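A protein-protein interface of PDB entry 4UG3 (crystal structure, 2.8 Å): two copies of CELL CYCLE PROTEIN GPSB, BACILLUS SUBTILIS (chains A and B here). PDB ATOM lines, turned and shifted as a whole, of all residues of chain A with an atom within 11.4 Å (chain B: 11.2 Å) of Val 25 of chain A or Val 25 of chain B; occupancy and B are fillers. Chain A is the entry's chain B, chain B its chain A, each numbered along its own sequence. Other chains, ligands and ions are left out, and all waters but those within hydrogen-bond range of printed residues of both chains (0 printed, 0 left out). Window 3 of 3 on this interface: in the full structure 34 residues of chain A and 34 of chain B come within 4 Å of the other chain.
Printed residues of chain A that touch a printed residue of chain B: Phe 21, Lys 22, Thr 23, Gly 24, Val 25, Arg 26, Gly 27, Tyr 28, Lys 29 and Gln 30. Of the 11 printed residues of chain B, 10 touch a printed residue of chain A. Among the printed residues, no Asp or Glu carboxylate lies within 4 Å of a Lys or Arg side-chain nitrogen of the other chain.
Among the printed residues, pairs that only touch across the chains: Phe 21 of chain A with Tyr 28 of chain B (3.6 Å), Lys 22 of chain A with Tyr 28 of chain B (3.6 Å), Thr 23 of chain A with Gly 27 of chain B (3.1 Å), Thr 23 of chain A with Lys 29 of chain B (3.98 Å), Gly 24 of chain A with Arg 26 of chain B (3.5 Å), Val 25 of chain A with Gly 24 of chain B (3.8 Å), Val 25 of chain A with Arg 26 of chain B (3.8 Å), Arg 26 of chain A with Val 25 of chain B (3.6 Å), Gly 27 of chain A with Thr 23 of chain B (3.4 Å), Gly 27 of chain A with Gly 27 of chain B (3.9 Å), Gly 27 of chain A with Tyr 28 of chain B (3.1 Å), Gly 27 of chain A with Gln 30 of chain B (3.98 Å), Tyr 28 of chain A with Phe 21 of chain B (3.6 Å), Tyr 28 of chain A with Lys 22 of chain B (3.4 Å), Tyr 28 of chain A with Gly 27 of chain B (3.0 Å), Tyr 28 of chain A with Gln 30 of chain B (3.5 Å), Lys 29 of chain A with Thr 23 of chain B (3.96 Å), Gln 30 of chain A with Gly 27 of chain B (3.7 Å) and Gln 30 of chain A with Tyr 28 of chain B (3.5 Å).
Gly 24 of chain A touches Gly 27 of chain B, and with the chains exchanged Gly 27 of chain A touches Gly 24 of chain B. Val 25 of chain A touches Arg 26 of chain B, and with the chains exchanged Arg 26 of chain A touches Val 25 of chain B. Arg 26 of chain A touches Gln 30 of chain B, but with the chains exchanged Gln 30 of chain A does not touch Arg 26 of chain B (4.4 Å). Gly 27 of chain A touches Tyr 28 of chain B, and with the chains exchanged Tyr 28 of chain A touches Gly 27 of chain B.
Of chain B, only Gly 24 (3.8 Å), Val 25 (2.3 Å) and Arg 26 (3.8 Å) come within 4 Å of Val 25 of chain A. Of chain A, only Val 25 and Arg 26 come within 4 Å of Val 25 of chain B. Arg 26 of chain A touches four residues of chain B. Of chain B, only Thr 23, Gly 24, Gly 27, Tyr 28 and Gln 30 come within 4 Å of Gly 27 of chain A. Thr 23 of chain B touches three residues of chain A. Gly 24 of chain B touches three residues of chain A. Of the printed residues of chain A, Arg 26 of chain B touches Thr 23, Gly 24 and Val 25. Printed residues of chain B within 4 Å of Lys 22 of chain A: Tyr 28 and Lys 29. Of the printed residues of chain B, Lys 29 of chain A touches Lys 22 (2.7 Å) and Thr 23 (3.96 Å). Of the printed residues of chain B, Phe 21 of chain A touches Tyr 28. Glu 31 of chain A touches none of the printed residues of chain B. Glu 31 of chain B touches none of the printed residues of chain A. The nearest printed residue of chain A that does not touch Phe 21 of chain B is Lys 29 of chain A (4.9 Å).
NZ of Lys 29 of chain B is in salt-bridge range of OE2 of Glu 31 of chain B, at 3.99 Å.
The backbone carbonyl oxygen (O) of Arg 26 of chain A lies within hydrogen-bond range of the side-chain amide nitrogen (NE2) of Gln 30 of chain B (2.8 Å). N of Lys 29 of chain A lies within hydrogen-bond range of O of Lys 22 of chain B (2.7 Å). O of Val 25 of chain A lies close to O of Val 25 of chain B, at 2.3 Å. The backbone carbonyl oxygen (O) of Gly 27 of chain B is in hydrogen-bond range of the backbone NH (N) of Gly 24 of chain A, 3.3 Å away. The backbone NH of Lys 29 of chain B is in hydrogen-bond range of the backbone carbonyl oxygen of Lys 22 of chain A (2.7 Å). The backbone carbonyl oxygen of Tyr 28 of chain B is in hydrogen-bond range of the backbone NH of Tyr 28 of chain A, 2.8 Å away. The guanidinium group (NE) of Arg 26 of chain A sits at hydrogen-bond distance from the backbone carbonyl oxygen (O) of Gly 24 of chain B (3.5 Å). The guanidinium group of Arg 26 of chain B is in hydrogen-bond range of the side-chain hydroxyl of Thr 23 of chain A (2.9 Å). The backbone NH of Gly 24 of chain B is in hydrogen-bond range of the backbone carbonyl oxygen of Gly 27 of chain A (3.2 Å). The side-chain hydroxyl (OG1) of Thr 23 of chain B lies within hydrogen-bond range of the guanidinium group (NE) of Arg 26 of chain A, 3.2 Å away.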
ATOM      1  N   PHE A  21     -22.139 -14.964 -19.081  1.00  0.00           N
ATOM      2  CA  PHE A  21     -21.581 -15.173 -20.407  1.00  0.00           C
ATOM      3  C   PHE A  21     -21.937 -16.536 -20.977  1.00  0.00           C
ATOM      4  O   PHE A  21     -22.223 -17.482 -20.241  1.00  0.00           O
ATOM      5  CB  PHE A  21     -20.067 -15.006 -20.395  1.00  0.00           C
ATOM      6  CG  PHE A  21     -19.624 -13.606 -20.107  1.00  0.00           C
ATOM      7  CD1 PHE A  21     -19.710 -12.615 -21.088  1.00  0.00           C
ATOM      8  CD2 PHE A  21     -19.135 -13.264 -18.862  1.00  0.00           C
ATOM      9  CE1 PHE A  21     -19.325 -11.312 -20.809  1.00  0.00           C
ATOM     10  CE2 PHE A  21     -18.740 -11.971 -18.593  1.00  0.00           C
ATOM     11  CZ  PHE A  21     -18.830 -10.992 -19.557  1.00  0.00           C
ATOM     12  N   LYS A  22     -21.932 -16.612 -22.307  1.00  0.00           N
ATOM     13  CA  LYS A  22     -21.967 -17.899 -23.009  1.00  0.00           C
ATOM     14  C   LYS A  22     -20.607 -18.575 -22.812  1.00  0.00           C
ATOM     15  O   LYS A  22     -19.579 -17.883 -22.740  1.00  0.00           O
ATOM     16  CB  LYS A  22     -22.272 -17.736 -24.516  1.00  0.00           C
ATOM     17  CG  LYS A  22     -23.588 -18.382 -24.970  1.00  0.00           C
ATOM     18  CD  LYS A  22     -23.522 -18.930 -26.412  1.00  0.00           C
ATOM     19  CE  LYS A  22     -24.746 -19.783 -26.753  1.00  0.00           C
ATOM     20  NZ  LYS A  22     -25.300 -19.474 -28.105  1.00  0.00           N
ATOM     21  N   THR A  23     -20.615 -19.911 -22.733  1.00  0.00           N
ATOM     22  CA  THR A  23     -19.393 -20.721 -22.669  1.00  0.00           C
ATOM     23  C   THR A  23     -19.069 -21.502 -23.955  1.00  0.00           C
ATOM     24  O   THR A  23     -19.901 -22.174 -24.488  1.00  0.00           O
ATOM     25  CB  THR A  23     -19.462 -21.695 -21.486  1.00  0.00           C
ATOM     26  OG1 THR A  23     -20.537 -22.589 -21.681  1.00  0.00           O
ATOM     27  CG2 THR A  23     -19.720 -20.944 -20.178  1.00  0.00           C
ATOM     28  N   GLY A  24     -17.844 -21.383 -24.441  1.00  0.00           N
ATOM     29  CA  GLY A  24     -17.339 -22.113 -25.601  1.00  0.00           C
ATOM     30  C   GLY A  24     -16.251 -23.090 -25.169  1.00  0.00           C
ATOM     31  O   GLY A  24     -15.881 -23.160 -23.985  1.00  0.00           O
ATOM     32  N   VAL A  25     -15.714 -23.832 -26.133  1.00  0.00           N
ATOM     33  CA  VAL A  25     -14.834 -24.955 -25.821  1.00  0.00           C
ATOM     34  C   VAL A  25     -13.430 -24.543 -25.472  1.00  0.00           C
ATOM     35  O   VAL A  25     -12.762 -25.297 -24.786  1.00  0.00           O
ATOM     36  CB  VAL A  25     -14.841 -26.071 -26.907  1.00  0.00           C
ATOM     37  CG1 VAL A  25     -13.470 -26.747 -27.088  1.00  0.00           C
ATOM     38  CG2 VAL A  25     -15.909 -27.127 -26.577  1.00  0.00           C
ATOM     39  N   ARG A  26     -12.933 -23.394 -25.904  1.00  0.00           N
ATOM     40  CA  ARG A  26     -11.639 -22.970 -25.331  1.00  0.00           C
ATOM     41  C   ARG A  26     -11.782 -21.512 -24.959  1.00  0.00           C
ATOM     42  O   ARG A  26     -11.073 -20.648 -25.421  1.00  0.00           O
ATOM     43  CB  ARG A  26     -10.455 -23.324 -26.251  1.00  0.00           C
ATOM     44  CG  ARG A  26      -9.099 -23.327 -25.558  1.00  0.00           C
ATOM     45  CD  ARG A  26      -8.554 -24.681 -25.100  1.00  0.00           C
ATOM     46  NE  ARG A  26      -7.979 -24.591 -23.753  1.00  0.00           N
ATOM     47  CZ  ARG A  26      -7.518 -25.618 -23.046  1.00  0.00           C
ATOM     48  NH1 ARG A  26      -7.506 -26.830 -23.550  1.00  0.00           N
ATOM     49  NH2 ARG A  26      -7.055 -25.449 -21.824  1.00  0.00           N
ATOM     50  N   GLY A  27     -12.763 -21.276 -24.096  1.00  0.00           N
ATOM     51  CA  GLY A  27     -13.039 -19.961 -23.556  1.00  0.00           C
ATOM     52  C   GLY A  27     -12.138 -19.657 -22.382  1.00  0.00           C
ATOM     53  O   GLY A  27     -11.356 -20.520 -21.930  1.00  0.00           O
ATOM     54  N   TYR A  28     -12.267 -18.416 -21.895  1.00  0.00           N
ATOM     55  CA  TYR A  28     -11.464 -17.871 -20.781  1.00  0.00           C
ATOM     56  C   TYR A  28     -11.802 -18.572 -19.497  1.00  0.00           C
ATOM     57  O   TYR A  28     -12.945 -18.901 -19.278  1.00  0.00           O
ATOM     58  CB  TYR A  28     -11.748 -16.369 -20.586  1.00  0.00           C
ATOM     59  CG  TYR A  28     -11.260 -15.438 -21.699  1.00  0.00           C
ATOM     60  CD1 TYR A  28      -9.988 -15.589 -22.295  1.00  0.00           C
ATOM     61  CD2 TYR A  28     -12.051 -14.373 -22.114  1.00  0.00           C
ATOM     62  CE1 TYR A  28      -9.550 -14.717 -23.289  1.00  0.00           C
ATOM     63  CE2 TYR A  28     -11.619 -13.504 -23.112  1.00  0.00           C
ATOM     64  CZ  TYR A  28     -10.383 -13.682 -23.693  1.00  0.00           C
ATOM     65  OH  TYR A  28     -10.017 -12.791 -24.657  1.00  0.00           O
ATOM     66  N   LYS A  29     -10.820 -18.786 -18.634  1.00  0.00           N
ATOM     67  CA  LYS A  29     -11.085 -19.295 -17.278  1.00  0.00           C
ATOM     68  C   LYS A  29     -12.104 -18.406 -16.545  1.00  0.00           C
ATOM     69  O   LYS A  29     -11.936 -17.195 -16.450  1.00  0.00           O
ATOM     70  CB  LYS A  29      -9.787 -19.346 -16.500  1.00  0.00           C
ATOM     71  CG  LYS A  29      -9.843 -20.025 -15.147  1.00  0.00           C
ATOM     72  CD  LYS A  29      -8.443 -20.513 -14.747  1.00  0.00           C
ATOM     73  CE  LYS A  29      -8.264 -20.588 -13.237  1.00  0.00           C
ATOM     74  NZ  LYS A  29      -7.004 -21.295 -12.895  1.00  0.00           N
ATOM     75  N   GLN A  30     -13.154 -19.011 -16.022  1.00  0.00           N
ATOM     76  CA  GLN A  30     -14.254 -18.248 -15.423  1.00  0.00           C
ATOM     77  C   GLN A  30     -13.854 -17.502 -14.141  1.00  0.00           C
ATOM     78  O   GLN A  30     -14.246 -16.379 -13.952  1.00  0.00           O
ATOM     79  CB  GLN A  30     -15.446 -19.164 -15.197  1.00  0.00           C
ATOM     80  CG  GLN A  30     -15.903 -19.788 -16.512  1.00  0.00           C
ATOM     81  CD  GLN A  30     -17.192 -20.585 -16.443  1.00  0.00           C
ATOM     82  OE1 GLN A  30     -17.460 -21.384 -17.317  1.00  0.00           O
ATOM     83  NE2 GLN A  30     -17.986 -20.366 -15.427  1.00  0.00           N
ATOM     84  N   GLU A  31     -13.010 -18.113 -13.322  1.00  0.00           N
ATOM     85  CA  GLU A  31     -12.496 -17.537 -12.070  1.00  0.00           C
ATOM     86  C   GLU A  31     -11.697 -16.258 -12.343  1.00  0.00           C
ATOM     87  O   GLU A  31     -11.828 -15.255 -11.615  1.00  0.00           O
ATOM     88  CB  GLU A  31     -11.573 -18.534 -11.328  1.00  0.00           C
ATOM     89  CG  GLU A  31     -12.153 -19.925 -10.962  1.00  0.00           C
ATOM     90  CD  GLU A  31     -12.161 -20.957 -12.124  1.00  0.00           C
ATOM     91  OE1 GLU A  31     -12.908 -20.751 -13.114  1.00  0.00           O
ATOM     92  OE2 GLU A  31     -11.429 -21.986 -12.055  1.00  0.00           O
ATOM     93  N   PHE B  21      -6.375 -13.579 -20.319  1.00  0.00           N
ATOM     94  CA  PHE B  21      -6.831 -14.568 -19.345  1.00  0.00           C
ATOM     95  C   PHE B  21      -6.384 -15.967 -19.735  1.00  0.00           C
ATOM     96  O   PHE B  21      -6.334 -16.306 -20.903  1.00  0.00           O
ATOM     97  CB  PHE B  21      -8.352 -14.558 -19.215  1.00  0.00           C
ATOM     98  CG  PHE B  21      -8.932 -13.244 -18.823  1.00  0.00           C
ATOM     99  CD1 PHE B  21      -9.029 -12.884 -17.486  1.00  0.00           C
ATOM    100  CD2 PHE B  21      -9.423 -12.369 -19.786  1.00  0.00           C
ATOM    101  CE1 PHE B  21      -9.592 -11.656 -17.106  1.00  0.00           C
ATOM    102  CE2 PHE B  21      -9.980 -11.141 -19.422  1.00  0.00           C
ATOM    103  CZ  PHE B  21     -10.071 -10.788 -18.074  1.00  0.00           C
ATOM    104  N   LYS B  22      -6.096 -16.798 -18.745  1.00  0.00           N
ATOM    105  CA  LYS B  22      -5.941 -18.220 -19.007  1.00  0.00           C
ATOM    106  C   LYS B  22      -7.211 -18.750 -19.633  1.00  0.00           C
ATOM    107  O   LYS B  22      -8.300 -18.183 -19.445  1.00  0.00           O
ATOM    108  CB  LYS B  22      -5.694 -19.001 -17.721  1.00  0.00           C
ATOM    109  CG  LYS B  22      -4.339 -18.744 -17.099  1.00  0.00           C
ATOM    110  CD  LYS B  22      -3.996 -19.746 -16.007  1.00  0.00           C
ATOM    111  CE  LYS B  22      -2.603 -20.328 -16.246  1.00  0.00           C
ATOM    112  NZ  LYS B  22      -2.050 -20.945 -15.016  1.00  0.00           N
ATOM    113  N   THR B  23      -7.053 -19.829 -20.387  1.00  0.00           N
ATOM    114  CA  THR B  23      -8.153 -20.624 -20.911  1.00  0.00           C
ATOM    115  C   THR B  23      -8.326 -21.932 -20.115  1.00  0.00           C
ATOM    116  O   THR B  23      -7.399 -22.409 -19.455  1.00  0.00           O
ATOM    117  CB  THR B  23      -7.903 -20.967 -22.382  1.00  0.00           C
ATOM    118  OG1 THR B  23      -6.822 -21.900 -22.486  1.00  0.00           O
ATOM    119  CG2 THR B  23      -7.550 -19.735 -23.164  1.00  0.00           C
ATOM    120  N   GLY B  24      -9.535 -22.482 -20.158  1.00  0.00           N
ATOM    121  CA  GLY B  24      -9.804 -23.834 -19.690  1.00  0.00           C
ATOM    122  C   GLY B  24     -10.374 -24.621 -20.832  1.00  0.00           C
ATOM    123  O   GLY B  24     -10.825 -24.059 -21.818  1.00  0.00           O
ATOM    124  N   VAL B  25     -10.390 -25.931 -20.704  1.00  0.00           N
ATOM    125  CA  VAL B  25     -11.151 -26.778 -21.645  1.00  0.00           C
ATOM    126  C   VAL B  25     -12.598 -26.258 -21.909  1.00  0.00           C
ATOM    127  O   VAL B  25     -13.163 -26.597 -22.912  1.00  0.00           O
ATOM    128  CB  VAL B  25     -11.177 -28.256 -21.161  1.00  0.00           C
ATOM    129  CG1 VAL B  25     -12.223 -29.083 -21.893  1.00  0.00           C
ATOM    130  CG2 VAL B  25      -9.818 -28.890 -21.361  1.00  0.00           C
ATOM    131  N   ARG B  26     -13.188 -25.487 -20.987  1.00  0.00           N
ATOM    132  CA  ARG B  26     -14.376 -24.664 -21.246  1.00  0.00           C
ATOM    133  C   ARG B  26     -14.372 -23.484 -20.296  1.00  0.00           C
ATOM    134  O   ARG B  26     -14.115 -23.645 -19.110  1.00  0.00           O
ATOM    135  CB  ARG B  26     -15.655 -25.475 -21.033  1.00  0.00           C
ATOM    136  CG  ARG B  26     -16.959 -24.679 -21.070  1.00  0.00           C
ATOM    137  CD  ARG B  26     -18.174 -25.582 -20.979  1.00  0.00           C
ATOM    138  NE  ARG B  26     -18.336 -26.317 -22.235  1.00  0.00           N
ATOM    139  CZ  ARG B  26     -19.052 -25.934 -23.295  1.00  0.00           C
ATOM    140  NH1 ARG B  26     -19.766 -24.806 -23.312  1.00  0.00           N
ATOM    141  NH2 ARG B  26     -19.050 -26.707 -24.377  1.00  0.00           N
ATOM    142  N   GLY B  27     -14.663 -22.296 -20.802  1.00  0.00           N
ATOM    143  CA  GLY B  27     -14.888 -21.123 -19.942  1.00  0.00           C
ATOM    144  C   GLY B  27     -15.755 -20.103 -20.680  1.00  0.00           C
ATOM    145  O   GLY B  27     -16.481 -20.465 -21.613  1.00  0.00           O
ATOM    146  N   TYR B  28     -15.673 -18.829 -20.300  1.00  0.00           N
ATOM    147  CA  TYR B  28     -16.467 -17.813 -20.965  1.00  0.00           C
ATOM    148  C   TYR B  28     -15.997 -17.636 -22.423  1.00  0.00           C
ATOM    149  O   TYR B  28     -14.797 -17.506 -22.699  1.00  0.00           O
ATOM    150  CB  TYR B  28     -16.476 -16.467 -20.211  1.00  0.00           C
ATOM    151  CG  TYR B  28     -16.980 -16.534 -18.794  1.00  0.00           C
ATOM    152  CD1 TYR B  28     -18.091 -17.334 -18.435  1.00  0.00           C
ATOM    153  CD2 TYR B  28     -16.347 -15.808 -17.785  1.00  0.00           C
ATOM    154  CE1 TYR B  28     -18.530 -17.401 -17.114  1.00  0.00           C
ATOM    155  CE2 TYR B  28     -16.787 -15.869 -16.466  1.00  0.00           C
ATOM    156  CZ  TYR B  28     -17.878 -16.660 -16.133  1.00  0.00           C
ATOM    157  OH  TYR B  28     -18.283 -16.723 -14.819  1.00  0.00           O
ATOM    158  N   LYS B  29     -16.975 -17.634 -23.341  1.00  0.00           N
ATOM    159  CA  LYS B  29     -16.730 -17.343 -24.755  1.00  0.00           C
ATOM    160  C   LYS B  29     -16.030 -16.001 -24.868  1.00  0.00           C
ATOM    161  O   LYS B  29     -16.523 -15.008 -24.356  1.00  0.00           O
ATOM    162  CB  LYS B  29     -18.028 -17.348 -25.574  1.00  0.00           C
ATOM    163  CG  LYS B  29     -17.795 -17.239 -27.067  1.00  0.00           C
ATOM    164  CD  LYS B  29     -18.990 -17.682 -27.901  1.00  0.00           C
ATOM    165  CE  LYS B  29     -18.814 -17.289 -29.373  1.00  0.00           C
ATOM    166  NZ  LYS B  29     -20.015 -17.528 -30.224  1.00  0.00           N
ATOM    167  N   GLN B  30     -14.906 -15.997 -25.569  1.00  0.00           N
ATOM    168  CA  GLN B  30     -13.943 -14.909 -25.515  1.00  0.00           C
ATOM    169  C   GLN B  30     -14.483 -13.660 -26.137  1.00  0.00           C
ATOM    170  O   GLN B  30     -14.270 -12.556 -25.621  1.00  0.00           O
ATOM    171  CB  GLN B  30     -12.608 -15.298 -26.169  1.00  0.00           C
ATOM    172  CG  GLN B  30     -12.050 -16.616 -25.622  1.00  0.00           C
ATOM    173  CD  GLN B  30     -10.582 -16.898 -25.917  1.00  0.00           C
ATOM    174  OE1 GLN B  30      -9.866 -16.081 -26.500  1.00  0.00           O
ATOM    175  NE2 GLN B  30     -10.118 -18.062 -25.478  1.00  0.00           N
ATOM    176  N   GLU B  31     -15.201 -13.853 -27.230  1.00  0.00           N
ATOM    177  CA  GLU B  31     -15.729 -12.771 -28.038  1.00  0.00           C
ATOM    178  C   GLU B  31     -16.735 -11.953 -27.249  1.00  0.00           C
ATOM    179  O   GLU B  31     -16.701 -10.740 -27.318  1.00  0.00           O
ATOM    180  CB  GLU B  31     -16.355 -13.310 -29.341  1.00  0.00           C
ATOM    181  CG  GLU B  31     -15.440 -14.241 -30.176  1.00  0.00           C
ATOM    182  CD  GLU B  31     -15.784 -15.752 -30.081  1.00  0.00           C
ATOM    183  OE1 GLU B  31     -15.504 -16.400 -29.028  1.00  0.00           O
ATOM    184  OE2 GLU B  31     -16.318 -16.299 -31.083  1.00  0.00           O
